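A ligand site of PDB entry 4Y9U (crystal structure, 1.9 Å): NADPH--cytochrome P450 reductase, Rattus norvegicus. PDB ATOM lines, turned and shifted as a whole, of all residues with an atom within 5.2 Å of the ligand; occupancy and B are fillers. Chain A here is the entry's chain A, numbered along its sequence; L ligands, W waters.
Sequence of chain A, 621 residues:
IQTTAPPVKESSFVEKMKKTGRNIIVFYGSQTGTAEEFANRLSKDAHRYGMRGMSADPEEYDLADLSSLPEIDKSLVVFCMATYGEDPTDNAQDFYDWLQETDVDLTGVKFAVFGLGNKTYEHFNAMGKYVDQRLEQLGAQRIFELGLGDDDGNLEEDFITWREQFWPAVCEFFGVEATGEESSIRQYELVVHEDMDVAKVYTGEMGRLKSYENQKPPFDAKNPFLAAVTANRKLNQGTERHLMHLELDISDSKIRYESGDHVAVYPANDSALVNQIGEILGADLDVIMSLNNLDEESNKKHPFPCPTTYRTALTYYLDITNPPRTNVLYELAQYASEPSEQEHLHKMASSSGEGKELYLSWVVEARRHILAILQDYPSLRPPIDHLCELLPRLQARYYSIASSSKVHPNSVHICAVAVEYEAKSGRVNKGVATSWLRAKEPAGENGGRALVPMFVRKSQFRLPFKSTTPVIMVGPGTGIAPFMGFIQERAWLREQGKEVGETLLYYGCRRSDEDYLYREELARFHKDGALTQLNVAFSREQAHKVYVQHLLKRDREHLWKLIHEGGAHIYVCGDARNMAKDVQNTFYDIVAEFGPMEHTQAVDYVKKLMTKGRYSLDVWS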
ATOM      1  N   ARG A 241       6.741 -15.851  10.413  1.00  0.00           N
ATOM      2  CA  ARG A 241       6.841 -14.400  10.523  1.00  0.00           C
ATOM      3  C   ARG A 241       7.335 -13.808   9.213  1.00  0.00           C
ATOM      4  O   ARG A 241       7.509 -14.523   8.223  1.00  0.00           O
ATOM      5  CB  ARG A 241       7.829 -14.041  11.641  1.00  0.00           C
ATOM      6  CG  ARG A 241       7.529 -14.709  12.981  1.00  0.00           C
ATOM      7  CD  ARG A 241       8.511 -14.255  14.064  1.00  0.00           C
ATOM      8  NE  ARG A 241       9.872 -14.697  13.790  1.00  0.00           N
ATOM      9  CZ  ARG A 241      10.959 -14.144  14.323  1.00  0.00           C
ATOM     10  NH1 ARG A 241      10.836 -13.115  15.156  1.00  0.00           N
ATOM     11  NH2 ARG A 241      12.169 -14.610  14.022  1.00  0.00           N
ATOM     12  N   LEU A 243      10.426 -11.330   7.915  1.00  0.00           N
ATOM     13  CA  LEU A 243      11.650 -10.574   8.171  1.00  0.00           C
ATOM     14  C   LEU A 243      12.093 -10.050   6.809  1.00  0.00           C
ATOM     15  O   LEU A 243      12.057 -10.787   5.814  1.00  0.00           O
ATOM     16  CB  LEU A 243      12.709 -11.450   8.824  1.00  0.00           C
ATOM     17  CG  LEU A 243      12.327 -11.836  10.270  1.00  0.00           C
ATOM     18  CD1 LEU A 243      11.648 -13.193  10.269  1.00  0.00           C
ATOM     19  CD2 LEU A 243      13.554 -11.864  11.167  1.00  0.00           C
ATOM     20  N   VAL A 417      12.253  -6.999  11.454  1.00  0.00           N
ATOM     21  CA  VAL A 417      11.180  -7.964  11.598  1.00  0.00           C
ATOM     22  C   VAL A 417       9.883  -7.159  11.628  1.00  0.00           C
ATOM     23  O   VAL A 417       9.766  -6.173  12.379  1.00  0.00           O
ATOM     24  CB  VAL A 417      11.325  -8.820  12.892  1.00  0.00           C
ATOM     25  CG1 VAL A 417      11.440  -7.925  14.121  1.00  0.00           C
ATOM     26  CG2 VAL A 417      10.140  -9.777  13.008  1.00  0.00           C
ATOM     27  N   PRO A 476      21.911 -12.659  17.584  1.00  0.00           N
ATOM     28  CA  PRO A 476      20.860 -13.574  17.123  1.00  0.00           C
ATOM     29  C   PRO A 476      19.641 -12.808  16.591  1.00  0.00           C
ATOM     30  O   PRO A 476      19.387 -11.665  16.976  1.00  0.00           O
ATOM     31  CB  PRO A 476      20.540 -14.379  18.377  1.00  0.00           C
ATOM     32  CG  PRO A 476      20.785 -13.396  19.482  1.00  0.00           C
ATOM     33  CD  PRO A 476      22.061 -12.723  19.053  1.00  0.00           C
ATOM     34  N   GLY A 477      18.877 -13.449  15.701  1.00  0.00           N
ATOM     35  CA  GLY A 477      17.720 -12.818  15.118  1.00  0.00           C
ATOM     36  C   GLY A 477      18.117 -11.551  14.391  1.00  0.00           C
ATOM     37  O   GLY A 477      19.170 -11.526  13.740  1.00  0.00           O
ATOM     38  N   THR A 478      17.297 -10.499  14.488  1.00  0.00           N
ATOM     39  CA  THR A 478      17.598  -9.230  13.827  1.00  0.00           C
ATOM     40  C   THR A 478      18.854  -8.576  14.398  1.00  0.00           C
ATOM     41  O   THR A 478      19.304  -7.542  13.917  1.00  0.00           O
ATOM     42  CB  THR A 478      16.420  -8.223  13.933  1.00  0.00           C
ATOM     43  OG1 THR A 478      15.996  -8.104  15.301  1.00  0.00           O
ATOM     44  CG2 THR A 478      15.260  -8.680  13.068  1.00  0.00           C
ATOM     45  N   GLY A 479      19.417  -9.178  15.439  1.00  0.00           N
ATOM     46  CA  GLY A 479      20.636  -8.642  16.001  1.00  0.00           C
ATOM     47  C   GLY A 479      21.807  -8.818  15.035  1.00  0.00           C
ATOM     48  O   GLY A 479      22.896  -8.305  15.258  1.00  0.00           O
ATOM     49  N   GLY A 508      22.033 -16.668  15.797  1.00  0.00           N
ATOM     50  CA  GLY A 508      20.986 -17.571  16.254  1.00  0.00           C
ATOM     51  C   GLY A 508      19.636 -17.318  15.604  1.00  0.00           C
ATOM     52  O   GLY A 508      19.281 -16.170  15.310  1.00  0.00           O
ATOM     53  N   CYS A 509      18.894 -18.391  15.355  1.00  0.00           N
ATOM     54  CA  CYS A 509      17.573 -18.306  14.770  1.00  0.00           C
ATOM     55  C   CYS A 509      16.808 -19.547  15.229  1.00  0.00           C
ATOM     56  O   CYS A 509      17.367 -20.398  15.911  1.00  0.00           O
ATOM     57  CB  CYS A 509      17.650 -18.250  13.229  1.00  0.00           C
ATOM     58  SG  CYS A 509      18.350 -19.711  12.418  1.00  0.00           S
ATOM     59  N   ARG A 510      15.527 -19.651  14.866  1.00  0.00           N
ATOM     60  CA  ARG A 510      14.726 -20.791  15.280  1.00  0.00           C
ATOM     61  C   ARG A 510      15.075 -22.084  14.547  1.00  0.00           C
ATOM     62  O   ARG A 510      15.345 -23.107  15.175  1.00  0.00           O
ATOM     63  CB  ARG A 510      13.241 -20.480  15.078  1.00  0.00           C
ATOM     64  CG  ARG A 510      12.751 -19.296  15.899  1.00  0.00           C
ATOM     65  CD  ARG A 510      11.289 -18.995  15.574  1.00  0.00           C
ATOM     66  NE  ARG A 510      10.778 -17.866  16.348  1.00  0.00           N
ATOM     67  CZ  ARG A 510       9.528 -17.434  16.288  1.00  0.00           C
ATOM     68  NH1 ARG A 510       8.639 -18.041  15.510  1.00  0.00           N
ATOM     69  NH2 ARG A 510       9.148 -16.402  17.020  1.00  0.00           N
ATOM     70  N   ASP A 515      13.937 -19.221   9.627  1.00  0.00           N
ATOM     71  CA  ASP A 515      14.347 -17.824   9.673  1.00  0.00           C
ATOM     72  C   ASP A 515      15.851 -17.567   9.828  1.00  0.00           C
ATOM     73  O   ASP A 515      16.273 -16.727  10.631  1.00  0.00           O
ATOM     74  CB  ASP A 515      13.567 -17.098  10.774  1.00  0.00           C
ATOM     75  CG  ASP A 515      13.661 -17.794  12.133  1.00  0.00           C
ATOM     76  OD1 ASP A 515      14.460 -18.737  12.258  1.00  0.00           O
ATOM     77  OD2 ASP A 515      12.932 -17.388  13.068  1.00  0.00           O
ATOM     78  N   ALA A 537      23.318 -20.912  16.424  1.00  0.00           N
ATOM     79  CA  ALA A 537      22.496 -21.657  17.366  1.00  0.00           C
ATOM     80  C   ALA A 537      21.063 -21.734  16.818  1.00  0.00           C
ATOM     81  O   ALA A 537      20.390 -20.719  16.668  1.00  0.00           O
ATOM     82  CB  ALA A 537      22.494 -20.954  18.714  1.00  0.00           C
ATOM     83  N   SER A 539      17.730 -22.521  17.818  1.00  0.00           N
ATOM     84  CA  SER A 539      16.987 -22.712  19.045  1.00  0.00           C
ATOM     85  C   SER A 539      15.837 -23.718  19.048  1.00  0.00           C
ATOM     86  O   SER A 539      15.506 -24.254  20.107  1.00  0.00           O
ATOM     87  CB  SER A 539      16.474 -21.369  19.567  1.00  0.00           C
ATOM     88  OG  SER A 539      15.465 -20.816  18.738  1.00  0.00           O
ATOM     89  N   ARG A 540      15.246 -23.994  17.899  1.00  0.00           N
ATOM     90  CA  ARG A 540      14.110 -24.905  17.866  1.00  0.00           C
ATOM     91  C   ARG A 540      14.282 -26.177  17.043  1.00  0.00           C
ATOM     92  O   ARG A 540      13.302 -26.856  16.723  1.00  0.00           O
ATOM     93  CB  ARG A 540      12.865 -24.135  17.395  1.00  0.00           C
ATOM     94  CG  ARG A 540      12.631 -22.851  18.198  1.00  0.00           C
ATOM     95  CD  ARG A 540      11.290 -22.157  17.929  1.00  0.00           C
ATOM     96  NE  ARG A 540      11.205 -20.909  18.681  1.00  0.00           N
ATOM     97  CZ  ARG A 540      10.105 -20.168  18.791  1.00  0.00           C
ATOM     98  NH1 ARG A 540       8.979 -20.543  18.192  1.00  0.00           N
ATOM     99  NH2 ARG A 540      10.122 -19.041  19.497  1.00  0.00           N
ATOM    100  N   LYS A 545      16.579 -25.795  24.154  1.00  0.00           N
ATOM    101  CA  LYS A 545      17.011 -24.573  23.489  1.00  0.00           C
ATOM    102  C   LYS A 545      18.533 -24.574  23.287  1.00  0.00           C
ATOM    103  O   LYS A 545      19.271 -25.060  24.143  1.00  0.00           O
ATOM    104  CB  LYS A 545      16.641 -23.348  24.325  1.00  0.00           C
ATOM    105  CG  LYS A 545      15.152 -23.108  24.524  1.00  0.00           C
ATOM    106  CD  LYS A 545      14.452 -22.756  23.225  1.00  0.00           C
ATOM    107  CE  LYS A 545      13.001 -22.357  23.474  1.00  0.00           C
ATOM    108  NZ  LYS A 545      12.293 -22.041  22.195  1.00  0.00           N
ATOM    109  N   TYR A 547      21.257 -21.649  22.304  1.00  0.00           N
ATOM    110  CA  TYR A 547      21.399 -20.210  22.084  1.00  0.00           C
ATOM    111  C   TYR A 547      22.846 -19.828  21.857  1.00  0.00           C
ATOM    112  O   TYR A 547      23.748 -20.611  22.100  1.00  0.00           O
ATOM    113  CB  TYR A 547      20.876 -19.440  23.306  1.00  0.00           C
ATOM    114  CG  TYR A 547      19.394 -19.567  23.602  1.00  0.00           C
ATOM    115  CD1 TYR A 547      18.443 -19.621  22.578  1.00  0.00           C
ATOM    116  CD2 TYR A 547      18.920 -19.525  24.920  1.00  0.00           C
ATOM    117  CE1 TYR A 547      17.076 -19.614  22.853  1.00  0.00           C
ATOM    118  CE2 TYR A 547      17.554 -19.516  25.205  1.00  0.00           C
ATOM    119  CZ  TYR A 547      16.641 -19.561  24.166  1.00  0.00           C
ATOM    120  OH  TYR A 547      15.284 -19.532  24.445  1.00  0.00           O
ATOM    121  N   VAL A 548      23.072 -18.597  21.418  1.00  0.00           N
ATOM    122  CA  VAL A 548      24.425 -18.155  21.159  1.00  0.00           C
ATOM    123  C   VAL A 548      25.335 -18.287  22.390  1.00  0.00           C
ATOM    124  O   VAL A 548      26.493 -18.703  22.254  1.00  0.00           O
ATOM    125  CB  VAL A 548      24.447 -16.702  20.620  1.00  0.00           C
ATOM    126  CG1 VAL A 548      23.879 -16.667  19.191  1.00  0.00           C
ATOM    127  CG2 VAL A 548      23.629 -15.770  21.525  1.00  0.00           C
ATOM    128  N   GLN A 549      24.835 -17.978  23.587  1.00  0.00           N
ATOM    129  CA  GLN A 549      25.691 -18.084  24.772  1.00  0.00           C
ATOM    130  C   GLN A 549      26.135 -19.520  25.055  1.00  0.00           C
ATOM    131  O   GLN A 549      27.144 -19.730  25.731  1.00  0.00           O
ATOM    132  CB  GLN A 549      25.006 -17.498  26.030  1.00  0.00           C
ATOM    133  CG  GLN A 549      23.686 -18.134  26.410  1.00  0.00           C
ATOM    134  CD  GLN A 549      22.513 -17.409  25.793  1.00  0.00           C
ATOM    135  OE1 GLN A 549      22.620 -16.867  24.682  1.00  0.00           O
ATOM    136  NE2 GLN A 549      21.392 -17.395  26.489  1.00  0.00           N
ATOM    137  N   ASN A 578      16.467 -10.014  27.521  1.00  0.00           N
ATOM    138  CA  ASN A 578      17.070 -11.229  28.069  1.00  0.00           C
ATOM    139  C   ASN A 578      18.379 -11.683  27.438  1.00  0.00           C
ATOM    140  O   ASN A 578      19.305 -12.068  28.133  1.00  0.00           O
ATOM    141  CB  ASN A 578      16.060 -12.381  27.999  1.00  0.00           C
ATOM    142  CG  ASN A 578      14.829 -12.117  28.842  1.00  0.00           C
ATOM    143  OD1 ASN A 578      13.841 -11.564  28.364  1.00  0.00           O
ATOM    144  ND2 ASN A 578      14.887 -12.507  30.112  1.00  0.00           N
ATOM    145  N   MET A 579      18.450 -11.653  26.111  1.00  0.00           N
ATOM    146  CA  MET A 579      19.655 -12.100  25.411  1.00  0.00           C
ATOM    147  C   MET A 579      20.920 -11.367  25.847  1.00  0.00           C
ATOM    148  O   MET A 579      21.889 -12.006  26.276  1.00  0.00           O
ATOM    149  CB  MET A 579      19.439 -11.957  23.894  1.00  0.00           C
ATOM    150  CG  MET A 579      20.579 -12.531  23.034  1.00  0.00           C
ATOM    151  SD  MET A 579      21.966 -11.401  22.872  1.00  0.00           S
ATOM    152  CE  MET A 579      21.216 -10.071  21.918  1.00  0.00           C
ATOM    153  N   ASP A 582      21.984 -12.452  29.308  1.00  0.00           N
ATOM    154  CA  ASP A 582      22.472 -13.830  29.367  1.00  0.00           C
ATOM    155  C   ASP A 582      23.862 -13.935  28.753  1.00  0.00           C
ATOM    156  O   ASP A 582      24.738 -14.636  29.276  1.00  0.00           O
ATOM    157  CB  ASP A 582      21.517 -14.789  28.643  1.00  0.00           C
ATOM    158  CG  ASP A 582      20.204 -14.982  29.372  1.00  0.00           C
ATOM    159  OD1 ASP A 582      20.174 -14.843  30.621  1.00  0.00           O
ATOM    160  OD2 ASP A 582      19.202 -15.298  28.699  1.00  0.00           O
HETATM  161  P1  LIG L   1      13.923 -13.868  17.774  1.00  0.00           P
HETATM  162  O1  LIG L   1      13.692 -14.638  16.529  1.00  0.00           O
HETATM  163  O2  LIG L   1      12.799 -13.657  18.708  1.00  0.00           O
HETATM  164  O3  LIG L   1      15.154 -14.533  18.570  1.00  0.00           O
HETATM  165  C1  LIG L   1      16.324 -14.901  17.819  1.00  0.00           C
HETATM  166  C2  LIG L   1      16.962 -16.133  18.453  1.00  0.00           C
HETATM  167  O4  LIG L   1      17.303 -15.792  19.816  1.00  0.00           O
HETATM  168  C3  LIG L   1      15.940 -17.257  18.532  1.00  0.00           C
HETATM  169  O5  LIG L   1      16.574 -18.507  18.228  1.00  0.00           O
HETATM  170  C4  LIG L   1      15.485 -17.221  19.985  1.00  0.00           C
HETATM  171  O6  LIG L   1      15.121 -18.546  20.405  1.00  0.00           O
HETATM  172  C5  LIG L   1      16.815 -16.865  20.631  1.00  0.00           C
HETATM  173  N1  LIG L   1      16.696 -16.439  22.047  1.00  0.00           N
HETATM  174  C6  LIG L   1      15.578 -16.250  22.738  1.00  0.00           C
HETATM  175  N2  LIG L   1      15.922 -15.910  23.976  1.00  0.00           N
HETATM  176  C7  LIG L   1      17.249 -15.888  24.058  1.00  0.00           C
HETATM  177  C8  LIG L   1      18.074 -15.647  25.070  1.00  0.00           C
HETATM  178  N3  LIG L   1      17.526 -15.405  26.256  1.00  0.00           N
HETATM  179  N4  LIG L   1      19.410 -15.695  24.921  1.00  0.00           N
HETATM  180  C9  LIG L   1      19.946 -16.006  23.671  1.00  0.00           C
HETATM  181  N5  LIG L   1      19.050 -16.269  22.626  1.00  0.00           N
HETATM  182  C10 LIG L   1      17.729 -16.210  22.855  1.00  0.00           C
HETATM  183  O7  LIG L   1      14.535 -12.442  17.378  1.00  0.00           O
HETATM  184  P2  LIG L   1      14.015 -11.031  16.815  1.00  0.00           P
HETATM  185  O8  LIG L   1      14.982 -10.510  15.821  1.00  0.00           O
HETATM  186  O9  LIG L   1      12.594 -11.166  16.437  1.00  0.00           O
HETATM  187  O10 LIG L   1      14.084 -10.085  18.126  1.00  0.00           O
HETATM  188  P3  LIG L   1      13.640 -18.919  20.910  1.00  0.00           P
HETATM  189  O11 LIG L   1      13.440 -20.280  20.368  1.00  0.00           O
HETATM  190  O12 LIG L   1      13.716 -18.850  22.389  1.00  0.00           O
HETATM  191  O13 LIG L   1      12.778 -17.878  20.297  1.00  0.00           O
HETATM  192  O   HOH W   1      12.090 -15.419  21.165  1.00  0.00           O
HETATM  193  O   HOH W   2      20.580 -17.287  20.507  1.00  0.00           O
HETATM  194  O   HOH W   3      17.447 -12.960  21.050  1.00  0.00           O
HETATM  195  O   HOH W   4      12.122 -16.569  18.060  1.00  0.00           O
HETATM  196  O   HOH W   5      14.919 -16.238  14.734  1.00  0.00           O
HETATM  197  O   HOH W   6      19.268 -19.064  18.734  1.00  0.00           O
HETATM  198  O   HOH W   7      16.676  -8.708  18.293  1.00  0.00           O
HETATM  199  O   HOH W   8      11.355 -18.660  23.745  1.00  0.00           O
HETATM  200  O   HOH W   9      14.947 -15.634  28.106  1.00  0.00           O
HETATM  201  O   HOH W  10      10.239  -9.990  17.408  1.00  0.00           O
HETATM  202  O   HOH W  11      10.505 -12.125  19.209  1.00  0.00           O
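The side-chain hydroxyl of Ser 539 sits at hydrogen-bond distance from an oxygen (O5) of the ligand, at 2.6 Å.
The backbone NH (N) of Thr 478 sits at hydrogen-bond distance from an oxygen (O8) of the ligand (2.7 Å).
OG1 of Thr 478 is in hydrogen-bond range of O8 of the ligand (2.7 Å).
The side-chain hydroxyl (OH) of Tyr 547 sits at hydrogen-bond distance from an oxygen (O12) of the ligand, 2.7 Å away.
An oxygen (O11) of the ligand is in salt-bridge range of the side-chain amino group of Lys 545.
The guanidinium group (NE) of Arg 540 is in salt-bridge range of an oxygen (O11) of the ligand.
O9 of the ligand lies within salt-bridge range of NH1 of Arg 241 (2.9 Å).
The side-chain carboxylate of Asp 582 sits at hydrogen-bond distance from a nitrogen (N3) of the ligand, at 3.0 Å.
NE2 of Gln 549 is in hydrogen-bond range of N4 of the ligand (3.0 Å).
O of Cys 509 sits at hydrogen-bond distance from O5 of the ligand (3.1 Å).
The backbone carbonyl oxygen of Cys 509 sits at hydrogen-bond distance from the backbone NH of Ser 539 (2.9 Å).
The backbone carbonyl oxygen (O) of Arg 510 sits at hydrogen-bond distance from the backbone NH (N) of Arg 540, at 2.9 Å.
NH2 of Arg 241 lies within salt-bridge range of OD2 of Asp 515, 3.0 Å away.
N of Cys 509 lies within hydrogen-bond range of O of Ala 537, at 3.1 Å.
The backbone NH (N) of Gly 477 is in hydrogen-bond range of the backbone carbonyl oxygen (O) of Gly 508 (2.8 Å).
NE of Arg 510 is in salt-bridge range of OD2 of Asp 515.
Residues that only touch the ligand: Pro 476 (3.8 Å), Gly 477 (3.6 Å), Gly 508 (3.9 Å), Arg 510 (3.7 Å), Asn 578 (3.8 Å) and Met 579 (3.6 Å).
15 residues have an atom within 4 Å of the ligand: Arg 241, Pro 476, Gly 477, Thr 478, Gly 508, Cys 509, Arg 510, Ser 539, Arg 540, Lys 545, Tyr 547, Gln 549, Asn 578, Met 579 and Asp 582.
Water W4 lies within hydrogen-bond range of NE of Arg 510 (2.5 Å), O13 of the ligand (2.7 Å) and NH2 of Arg 540 (3.5 Å).
Water W5 lies within hydrogen-bond range of O1 of the ligand (2.7 Å), OD2 of Asp 515 (2.8 Å), NH2 of Arg 241 (3.3 Å) and N of Arg 510 (3.5 Å).
Water W6 lies within hydrogen-bond range of an oxygen (O5) of the ligand, the backbone carbonyl oxygen of Ala 537 and the backbone NH of Cys 509.
Water W2 bridges N5 of the ligand (2.8 Å) and N of Val 548 (3.0 Å).
Water W7 bridges an oxygen (O10) of the ligand (2.9 Å) and the side-chain hydroxyl of Thr 478 (3.1 Å).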
